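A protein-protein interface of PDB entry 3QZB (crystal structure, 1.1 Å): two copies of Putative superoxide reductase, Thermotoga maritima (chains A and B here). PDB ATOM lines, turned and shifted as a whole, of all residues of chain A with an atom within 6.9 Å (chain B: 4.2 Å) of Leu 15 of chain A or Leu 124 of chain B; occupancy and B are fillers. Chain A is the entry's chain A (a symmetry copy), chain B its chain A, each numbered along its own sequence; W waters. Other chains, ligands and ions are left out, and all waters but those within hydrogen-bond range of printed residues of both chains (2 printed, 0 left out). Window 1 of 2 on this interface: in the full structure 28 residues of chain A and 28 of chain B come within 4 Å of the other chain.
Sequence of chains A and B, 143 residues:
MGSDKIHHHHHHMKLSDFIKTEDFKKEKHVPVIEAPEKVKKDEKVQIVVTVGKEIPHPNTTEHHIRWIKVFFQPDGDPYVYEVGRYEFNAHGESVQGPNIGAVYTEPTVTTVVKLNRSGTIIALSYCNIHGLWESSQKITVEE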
ATOM      1  N   MET A  13      25.486  31.384  -5.389  1.00  0.00           N
ATOM      2  CA  MET A  13      26.291  30.781  -4.330  1.00  0.00           C
ATOM      3  C   MET A  13      25.989  29.322  -4.158  1.00  0.00           C
ATOM      4  O   MET A  13      24.852  28.969  -3.968  1.00  0.00           O
ATOM      5  CB  MET A  13      25.978  31.498  -3.005  1.00  0.00           C
ATOM      6  CG  MET A  13      26.891  31.003  -1.870  1.00  0.00           C
ATOM      7  SD  MET A  13      26.774  31.979  -0.428  1.00  0.00           S
ATOM      8  CE  MET A  13      27.545  33.508  -0.897  1.00  0.00           C
ATOM      9  N   LYS A  14      27.041  28.503  -4.146  1.00  0.00           N
ATOM     10  CA  LYS A  14      26.998  27.087  -3.895  1.00  0.00           C
ATOM     11  C   LYS A  14      27.578  26.818  -2.532  1.00  0.00           C
ATOM     12  O   LYS A  14      28.559  27.446  -2.111  1.00  0.00           O
ATOM     13  CB  LYS A  14      27.872  26.349  -4.896  1.00  0.00           C
ATOM     14  CG  LYS A  14      27.426  26.515  -6.320  1.00  0.00           C
ATOM     15  CD  LYS A  14      26.017  25.960  -6.519  1.00  0.00           C
ATOM     16  CE  LYS A  14      25.466  26.261  -7.914  1.00  0.00           C
ATOM     17  NZ  LYS A  14      24.622  27.476  -7.924  1.00  0.00           N
ATOM     18  N   LEU A  15      27.015  25.835  -1.858  1.00  0.00           N
ATOM     19  CA  LEU A  15      27.504  25.461  -0.548  1.00  0.00           C
ATOM     20  C   LEU A  15      28.979  25.105  -0.606  1.00  0.00           C
ATOM     21  O   LEU A  15      29.703  25.378   0.381  1.00  0.00           O
ATOM     22  CB  LEU A  15      26.674  24.302   0.022  1.00  0.00           C
ATOM     23  CG  LEU A  15      26.958  23.944   1.488  1.00  0.00           C
ATOM     24  CD1 LEU A  15      26.665  25.096   2.437  1.00  0.00           C
ATOM     25  CD2 LEU A  15      26.115  22.715   1.900  1.00  0.00           C
ATOM     26  N   SER A  16      29.444  24.528  -1.692  1.00  0.00           N
ATOM     27  CA  SER A  16      30.805  24.057  -1.629  1.00  0.00           C
ATOM     28  C   SER A  16      31.821  25.209  -1.690  1.00  0.00           C
ATOM     29  O   SER A  16      32.991  24.971  -1.379  1.00  0.00           O
ATOM     30  CB  SER A  16      31.005  23.045  -2.716  1.00  0.00           C
ATOM     31  OG  SER A  16      30.644  23.635  -3.963  1.00  0.00           O
ATOM     32  N   ASP A  17      31.382  26.447  -1.973  1.00  0.00           N
ATOM     33  CA  ASP A  17      32.229  27.607  -1.836  1.00  0.00           C
ATOM     34  C   ASP A  17      32.621  27.847  -0.341  1.00  0.00           C
ATOM     35  O   ASP A  17      33.555  28.608  -0.040  1.00  0.00           O
ATOM     36  CB  ASP A  17      31.500  28.868  -2.389  1.00  0.00           C
ATOM     37  CG  ASP A  17      31.168  28.795  -3.859  1.00  0.00           C
ATOM     38  OD1 ASP A  17      31.855  28.031  -4.575  1.00  0.00           O
ATOM     39  OD2 ASP A  17      30.184  29.520  -4.226  1.00  0.00           O
ATOM     40  N   PHE A  18      31.907  27.182   0.565  1.00  0.00           N
ATOM     41  CA  PHE A  18      32.076  27.301   1.987  1.00  0.00           C
ATOM     42  C   PHE A  18      32.342  25.988   2.670  1.00  0.00           C
ATOM     43  O   PHE A  18      32.071  25.821   3.863  1.00  0.00           O
ATOM     44  CB  PHE A  18      30.867  28.074   2.569  1.00  0.00           C
ATOM     45  CG  PHE A  18      30.837  29.462   2.070  1.00  0.00           C
ATOM     46  CD1 PHE A  18      31.558  30.444   2.713  1.00  0.00           C
ATOM     47  CD2 PHE A  18      30.186  29.793   0.898  1.00  0.00           C
ATOM     48  CE1 PHE A  18      31.631  31.720   2.216  1.00  0.00           C
ATOM     49  CE2 PHE A  18      30.247  31.090   0.389  1.00  0.00           C
ATOM     50  CZ  PHE A  18      30.981  32.043   1.051  1.00  0.00           C
ATOM     51  N   ILE A  19      32.840  24.978   1.951  1.00  0.00           N
ATOM     52  CA  ILE A  19      33.303  23.711   2.551  1.00  0.00           C
ATOM     53  C   ILE A  19      34.782  23.662   2.300  1.00  0.00           C
ATOM     54  O   ILE A  19      35.203  23.659   1.152  1.00  0.00           O
ATOM     55  CB  ILE A  19      32.601  22.454   1.945  1.00  0.00           C
ATOM     56  CG1 ILE A  19      31.084  22.550   2.102  1.00  0.00           C
ATOM     57  CG2 ILE A  19      33.170  21.174   2.573  1.00  0.00           C
ATOM     58  CD1 ILE A  19      30.315  21.448   1.356  1.00  0.00           C
ATOM     59  N   LYS A  20      35.570  23.657   3.357  1.00  0.00           N
ATOM     60  CA  LYS A  20      37.000  23.773   3.253  1.00  0.00           C
ATOM     61  C   LYS A  20      37.675  22.404   3.396  1.00  0.00           C
ATOM     62  O   LYS A  20      37.304  21.571   4.190  1.00  0.00           O
ATOM     63  CB  LYS A  20      37.521  24.737   4.309  1.00  0.00           C
ATOM     64  CG  LYS A  20      37.028  26.146   4.097  1.00  0.00           C
ATOM     65  CD  LYS A  20      37.496  27.215   5.091  1.00  0.00           C
ATOM     66  CE  LYS A  20      36.801  28.565   4.811  1.00  0.00           C
ATOM     67  NZ  LYS A  20      37.138  29.133   3.461  1.00  0.00           N
ATOM     68  N   LYS A  69      29.232  14.292   9.798  1.00  0.00           N
ATOM     69  CA  LYS A  69      28.421  13.353   9.036  1.00  0.00           C
ATOM     70  C   LYS A  69      29.290  12.665   8.062  1.00  0.00           C
ATOM     71  O   LYS A  69      30.351  13.155   7.662  1.00  0.00           O
ATOM     72  CB  LYS A  69      27.134  13.977   8.475  1.00  0.00           C
ATOM     73  CG  LYS A  69      27.324  15.034   7.443  1.00  0.00           C
ATOM     74  CD  LYS A  69      26.003  15.500   6.823  1.00  0.00           C
ATOM     75  CE  LYS A  69      24.906  15.937   7.777  1.00  0.00           C
ATOM     76  NZ  LYS A  69      25.318  16.985   8.782  1.00  0.00           N
ATOM     77  N   PHE A  71      29.243  10.396   4.366  1.00  0.00           N
ATOM     78  CA  PHE A  71      28.599   9.971   3.140  1.00  0.00           C
ATOM     79  C   PHE A  71      29.418   8.823   2.518  1.00  0.00           C
ATOM     80  O   PHE A  71      30.640   8.770   2.655  1.00  0.00           O
ATOM     81  CB  PHE A  71      28.495  11.114   2.128  1.00  0.00           C
ATOM     82  CG  PHE A  71      27.522  12.201   2.572  1.00  0.00           C
ATOM     83  CD1 PHE A  71      26.175  12.123   2.242  1.00  0.00           C
ATOM     84  CD2 PHE A  71      27.981  13.312   3.275  1.00  0.00           C
ATOM     85  CE1 PHE A  71      25.298  13.075   2.650  1.00  0.00           C
ATOM     86  CE2 PHE A  71      27.089  14.324   3.682  1.00  0.00           C
ATOM     87  CZ  PHE A  71      25.760  14.204   3.345  1.00  0.00           C
ATOM     88  N   LEU A 124      32.187  15.102   6.540  1.00  0.00           N
ATOM     89  CA  LEU A 124      31.865  16.540   6.600  1.00  0.00           C
ATOM     90  C   LEU A 124      31.687  16.877   8.065  1.00  0.00           C
ATOM     91  O   LEU A 124      30.949  16.216   8.792  1.00  0.00           O
ATOM     92  CB  LEU A 124      30.585  16.800   5.848  1.00  0.00           C
ATOM     93  CG  LEU A 124      30.133  18.272   5.701  1.00  0.00           C
ATOM     94  CD1 LEU A 124      30.995  19.028   4.791  1.00  0.00           C
ATOM     95  CD2 LEU A 124      28.664  18.333   5.278  1.00  0.00           C
ATOM     96  N   LEU A 132      32.154  24.719   7.736  1.00  0.00           N
ATOM     97  CA  LEU A 132      32.202  23.366   7.222  1.00  0.00           C
ATOM     98  C   LEU A 132      33.588  22.978   6.705  1.00  0.00           C
ATOM     99  O   LEU A 132      34.294  23.770   6.047  1.00  0.00           O
ATOM    100  CB  LEU A 132      31.219  23.223   6.036  1.00  0.00           C
ATOM    101  CG  LEU A 132      29.726  23.313   6.442  1.00  0.00           C
ATOM    102  CD1 LEU A 132      28.874  23.418   5.120  1.00  0.00           C
ATOM    103  CD2 LEU A 132      29.269  22.152   7.256  1.00  0.00           C
ATOM    104  N   ILE B  19      26.453  17.397  -5.113  1.00  0.00           N
ATOM    105  CA  ILE B  19      25.337  18.274  -4.704  1.00  0.00           C
ATOM    106  C   ILE B  19      24.839  18.909  -5.969  1.00  0.00           C
ATOM    107  O   ILE B  19      25.587  19.613  -6.631  1.00  0.00           O
ATOM    108  CB  ILE B  19      25.763  19.366  -3.671  1.00  0.00           C
ATOM    109  CG1 ILE B  19      26.373  18.726  -2.425  1.00  0.00           C
ATOM    110  CG2 ILE B  19      24.571  20.272  -3.336  1.00  0.00           C
ATOM    111  CD1 ILE B  19      26.995  19.740  -1.452  1.00  0.00           C
ATOM    112  N   TRP B  67      15.459  14.951   4.675  1.00  0.00           N
ATOM    113  CA  TRP B  67      15.707  16.212   5.395  1.00  0.00           C
ATOM    114  C   TRP B  67      15.931  17.350   4.469  1.00  0.00           C
ATOM    115  O   TRP B  67      16.286  17.202   3.311  1.00  0.00           O
ATOM    116  CB  TRP B  67      16.827  16.037   6.448  1.00  0.00           C
ATOM    117  CG  TRP B  67      18.160  15.503   5.990  1.00  0.00           C
ATOM    118  CD1 TRP B  67      18.633  14.250   6.248  1.00  0.00           C
ATOM    119  CD2 TRP B  67      19.205  16.141   5.191  1.00  0.00           C
ATOM    120  NE1 TRP B  67      19.896  14.090   5.782  1.00  0.00           N
ATOM    121  CE2 TRP B  67      20.286  15.227   5.119  1.00  0.00           C
ATOM    122  CE3 TRP B  67      19.355  17.372   4.564  1.00  0.00           C
ATOM    123  CZ2 TRP B  67      21.480  15.522   4.466  1.00  0.00           C
ATOM    124  CZ3 TRP B  67      20.525  17.660   3.917  1.00  0.00           C
ATOM    125  CH2 TRP B  67      21.578  16.747   3.882  1.00  0.00           C
ATOM    126  N   ILE B  68      15.785  18.546   5.074  1.00  0.00           N
ATOM    127  CA  ILE B  68      16.246  19.825   4.557  1.00  0.00           C
ATOM    128  C   ILE B  68      17.116  20.428   5.664  1.00  0.00           C
ATOM    129  O   ILE B  68      16.733  20.343   6.845  1.00  0.00           O
ATOM    130  CB  ILE B  68      15.059  20.743   4.276  1.00  0.00           C
ATOM    131  CG1 ILE B  68      14.300  20.293   3.024  1.00  0.00           C
ATOM    132  CG2 ILE B  68      15.511  22.226   4.161  1.00  0.00           C
ATOM    133  CD1 ILE B  68      12.886  20.842   2.948  1.00  0.00           C
ATOM    134  N   LYS B  69      18.254  21.012   5.303  1.00  0.00           N
ATOM    135  CA  LYS B  69      18.961  21.888   6.225  1.00  0.00           C
ATOM    136  C   LYS B  69      19.139  23.204   5.580  1.00  0.00           C
ATOM    137  O   LYS B  69      19.130  23.344   4.353  1.00  0.00           O
ATOM    138  CB  LYS B  69      20.224  21.250   6.824  1.00  0.00           C
ATOM    139  CG  LYS B  69      21.324  20.965   5.860  1.00  0.00           C
ATOM    140  CD  LYS B  69      22.601  20.473   6.549  1.00  0.00           C
ATOM    141  CE  LYS B  69      22.465  19.299   7.500  1.00  0.00           C
ATOM    142  NZ  LYS B  69      21.779  18.086   6.921  1.00  0.00           N
ATOM    143  N   PHE B  71      21.484  26.849   5.720  1.00  0.00           N
ATOM    144  CA  PHE B  71      22.660  27.593   6.124  1.00  0.00           C
ATOM    145  C   PHE B  71      22.424  29.090   5.844  1.00  0.00           C
ATOM    146  O   PHE B  71      21.724  29.455   4.900  1.00  0.00           O
ATOM    147  CB  PHE B  71      23.908  27.135   5.366  1.00  0.00           C
ATOM    148  CG  PHE B  71      24.343  25.725   5.754  1.00  0.00           C
ATOM    149  CD1 PHE B  71      25.220  25.522   6.813  1.00  0.00           C
ATOM    150  CD2 PHE B  71      23.904  24.627   5.021  1.00  0.00           C
ATOM    151  CE1 PHE B  71      25.597  24.270   7.178  1.00  0.00           C
ATOM    152  CE2 PHE B  71      24.308  23.322   5.368  1.00  0.00           C
ATOM    153  CZ  PHE B  71      25.169  23.161   6.431  1.00  0.00           C
ATOM    154  N   ILE B 122      21.056  29.359   2.091  1.00  0.00           N
ATOM    155  CA  ILE B 122      21.359  28.162   1.311  1.00  0.00           C
ATOM    156  C   ILE B 122      20.531  27.005   1.868  1.00  0.00           C
ATOM    157  O   ILE B 122      20.554  26.735   3.063  1.00  0.00           O
ATOM    158  CB  ILE B 122      22.853  27.823   1.324  1.00  0.00           C
ATOM    159  CG1 ILE B 122      23.743  28.990   0.829  1.00  0.00           C
ATOM    160  CG2 ILE B 122      23.105  26.587   0.455  1.00  0.00           C
ATOM    161  CD1 ILE B 122      25.230  28.742   1.070  1.00  0.00           C
ATOM    162  N   ALA B 123      19.762  26.360   0.999  1.00  0.00           N
ATOM    163  CA  ALA B 123      19.000  25.169   1.359  1.00  0.00           C
ATOM    164  C   ALA B 123      19.700  23.941   0.742  1.00  0.00           C
ATOM    165  O   ALA B 123      20.103  23.972  -0.432  1.00  0.00           O
ATOM    166  CB  ALA B 123      17.572  25.264   0.826  1.00  0.00           C
ATOM    167  N   LEU B 124      19.819  22.910   1.568  1.00  0.00           N
ATOM    168  CA  LEU B 124      20.380  21.614   1.139  1.00  0.00           C
ATOM    169  C   LEU B 124      19.362  20.561   1.523  1.00  0.00           C
ATOM    170  O   LEU B 124      18.896  20.501   2.659  1.00  0.00           O
ATOM    171  CB  LEU B 124      21.681  21.367   1.859  1.00  0.00           C
ATOM    172  CG  LEU B 124      22.483  20.104   1.464  1.00  0.00           C
ATOM    173  CD1 LEU B 124      23.072  20.218   0.130  1.00  0.00           C
ATOM    174  CD2 LEU B 124      23.537  19.795   2.530  1.00  0.00           C
ATOM    175  N   SER B 125      19.017  19.677   0.577  1.00  0.00           N
ATOM    176  CA  SER B 125      18.082  18.600   0.878  1.00  0.00           C
ATOM    177  C   SER B 125      18.629  17.262   0.435  1.00  0.00           C
ATOM    178  O   SER B 125      19.530  17.213  -0.435  1.00  0.00           O
ATOM    179  CB  SER B 125      16.721  18.876   0.245  1.00  0.00           C
ATOM    180  OG  SER B 125      16.828  19.006  -1.139  1.00  0.00           O
ATOM    181  N   TRP B 133      20.826  17.956  -3.004  1.00  0.00           N
ATOM    182  CA  TRP B 133      20.324  19.018  -3.851  1.00  0.00           C
ATOM    183  C   TRP B 133      20.401  20.319  -3.086  1.00  0.00           C
ATOM    184  O   TRP B 133      20.212  20.345  -1.871  1.00  0.00           O
ATOM    185  CB  TRP B 133      18.835  18.723  -4.200  1.00  0.00           C
ATOM    186  CG  TRP B 133      18.698  17.434  -4.929  1.00  0.00           C
ATOM    187  CD1 TRP B 133      18.714  16.177  -4.375  1.00  0.00           C
ATOM    188  CD2 TRP B 133      18.679  17.234  -6.342  1.00  0.00           C
ATOM    189  NE1 TRP B 133      18.658  15.231  -5.368  1.00  0.00           N
ATOM    190  CE2 TRP B 133      18.685  15.856  -6.575  1.00  0.00           C
ATOM    191  CE3 TRP B 133      18.689  18.107  -7.433  1.00  0.00           C
ATOM    192  CZ2 TRP B 133      18.612  15.317  -7.878  1.00  0.00           C
ATOM    193  CZ3 TRP B 133      18.632  17.587  -8.704  1.00  0.00           C
ATOM    194  CH2 TRP B 133      18.631  16.211  -8.929  1.00  0.00           C
ATOM    195  N   GLU B 134      20.613  21.423  -3.807  1.00  0.00           N
ATOM    196  CA  GLU B 134      20.716  22.744  -3.165  1.00  0.00           C
ATOM    197  C   GLU B 134      20.060  23.848  -3.947  1.00  0.00           C
ATOM    198  O   GLU B 134      19.822  23.728  -5.171  1.00  0.00           O
ATOM    199  CB  GLU B 134      22.177  23.120  -2.873  1.00  0.00           C
ATOM    200  CG  GLU B 134      23.003  23.413  -4.060  1.00  0.00           C
ATOM    201  CD  GLU B 134      24.398  23.870  -3.672  1.00  0.00           C
ATOM    202  OE1 GLU B 134      24.572  24.679  -2.753  1.00  0.00           O
ATOM    203  OE2 GLU B 134      25.328  23.508  -4.377  1.00  0.00           O
HETATM  204  O   HOH W   1      27.781  23.001  -3.535  1.00  0.00           O
HETATM  205  O   HOH W   2      23.040  26.843  -3.536  1.00  0.00           O
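The side-chain carboxylate of Glu 134 of chain B lies within hydrogen-bond range of the backbone NH of Leu 15 of chain A (2.8 Å).
O of Leu 124 of chain B lies within hydrogen-bond range of N of Lys 69 of chain B, at 2.8 Å. The backbone NH (N) of Phe 71 of chain B lies within hydrogen-bond range of the backbone carbonyl oxygen (O) of Ile 122 of chain B (2.8 Å). N of Lys 14 of chain A sits at hydrogen-bond distance from OD2 of Asp 17 of chain A (3.3 Å). N of Lys 20 of chain A lies within hydrogen-bond range of O of Leu 132 of chain A. The backbone NH of Lys 69 of chain A lies within hydrogen-bond range of the backbone carbonyl oxygen of Leu 124 of chain A.
Among the printed residues, pairs that only touch across the chains: Lys 14 of chain A with Glu 134 of chain B (3.3 Å), Leu 15 of chain A with Phe 71 of chain B (3.8 Å), Met 13 of chain A with Ile 122 of chain B (3.9 Å), Lys 69 of chain A with Lys 69 of chain B (3.9 Å), Leu 132 of chain A with Phe 71 of chain B (3.9 Å) and Leu 15 of chain A with Leu 124 of chain B (3.9 Å).
Printed residues of chain B within 4 Å of Met 13 of chain A: Ile 122 (3.9 Å). Leu 15 of chain A touches three residues of chain B. Leu 124 of chain B touches just one residue of chain A: Leu 15. Printed residues of chain A within 4 Å of Glu 134 of chain B: Lys 14 (3.3 Å) and Leu 15 (2.8 Å). The nearest residue of chain B that does not touch Leu 15 of chain A is Ile 122 of chain B (4.1 Å). The nearest residue of chain A that does not touch Leu 124 of chain B is Leu 124 of chain A (6.0 Å).
Printed residues of chain A that touch a printed residue of chain B: Met 13, Lys 14, Leu 15, Lys 69 and Leu 132. Hydrophobic or aromatic side chains of chain A that line the printed part of chain B: Met 13, Leu 15 and Leu 132. Hydrophobic or aromatic side chains of chain B within 4 Å of the printed part of chain A: Phe 71, Ile 122 and Leu 124. Along chain B the printed residues that touch a printed residue of chain A span positions 69 to 134. Among the printed residues, 7 pairs touch across the chains. Among the printed residues, no Asp or Glu carboxylate lies within 4 Å of a Lys or Arg side-chain nitrogen of the other chain.
Lys 69 of chain B touches its own counterpart, Lys 69 of chain A. Of the 7 pairs that touch across the chains among the printed residues, 1 has its exchanged pair printed and touching as well.
Water W1 lies within hydrogen-bond range of OE2 of Glu 134 of chain B (2.6 Å), N of Ser 16 of chain A (2.9 Å) and N of Leu 15 of chain A (3.4 Å). Water W2 bridges OE1 of Glu 134 of chain B and O of Met 13 of chain A.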
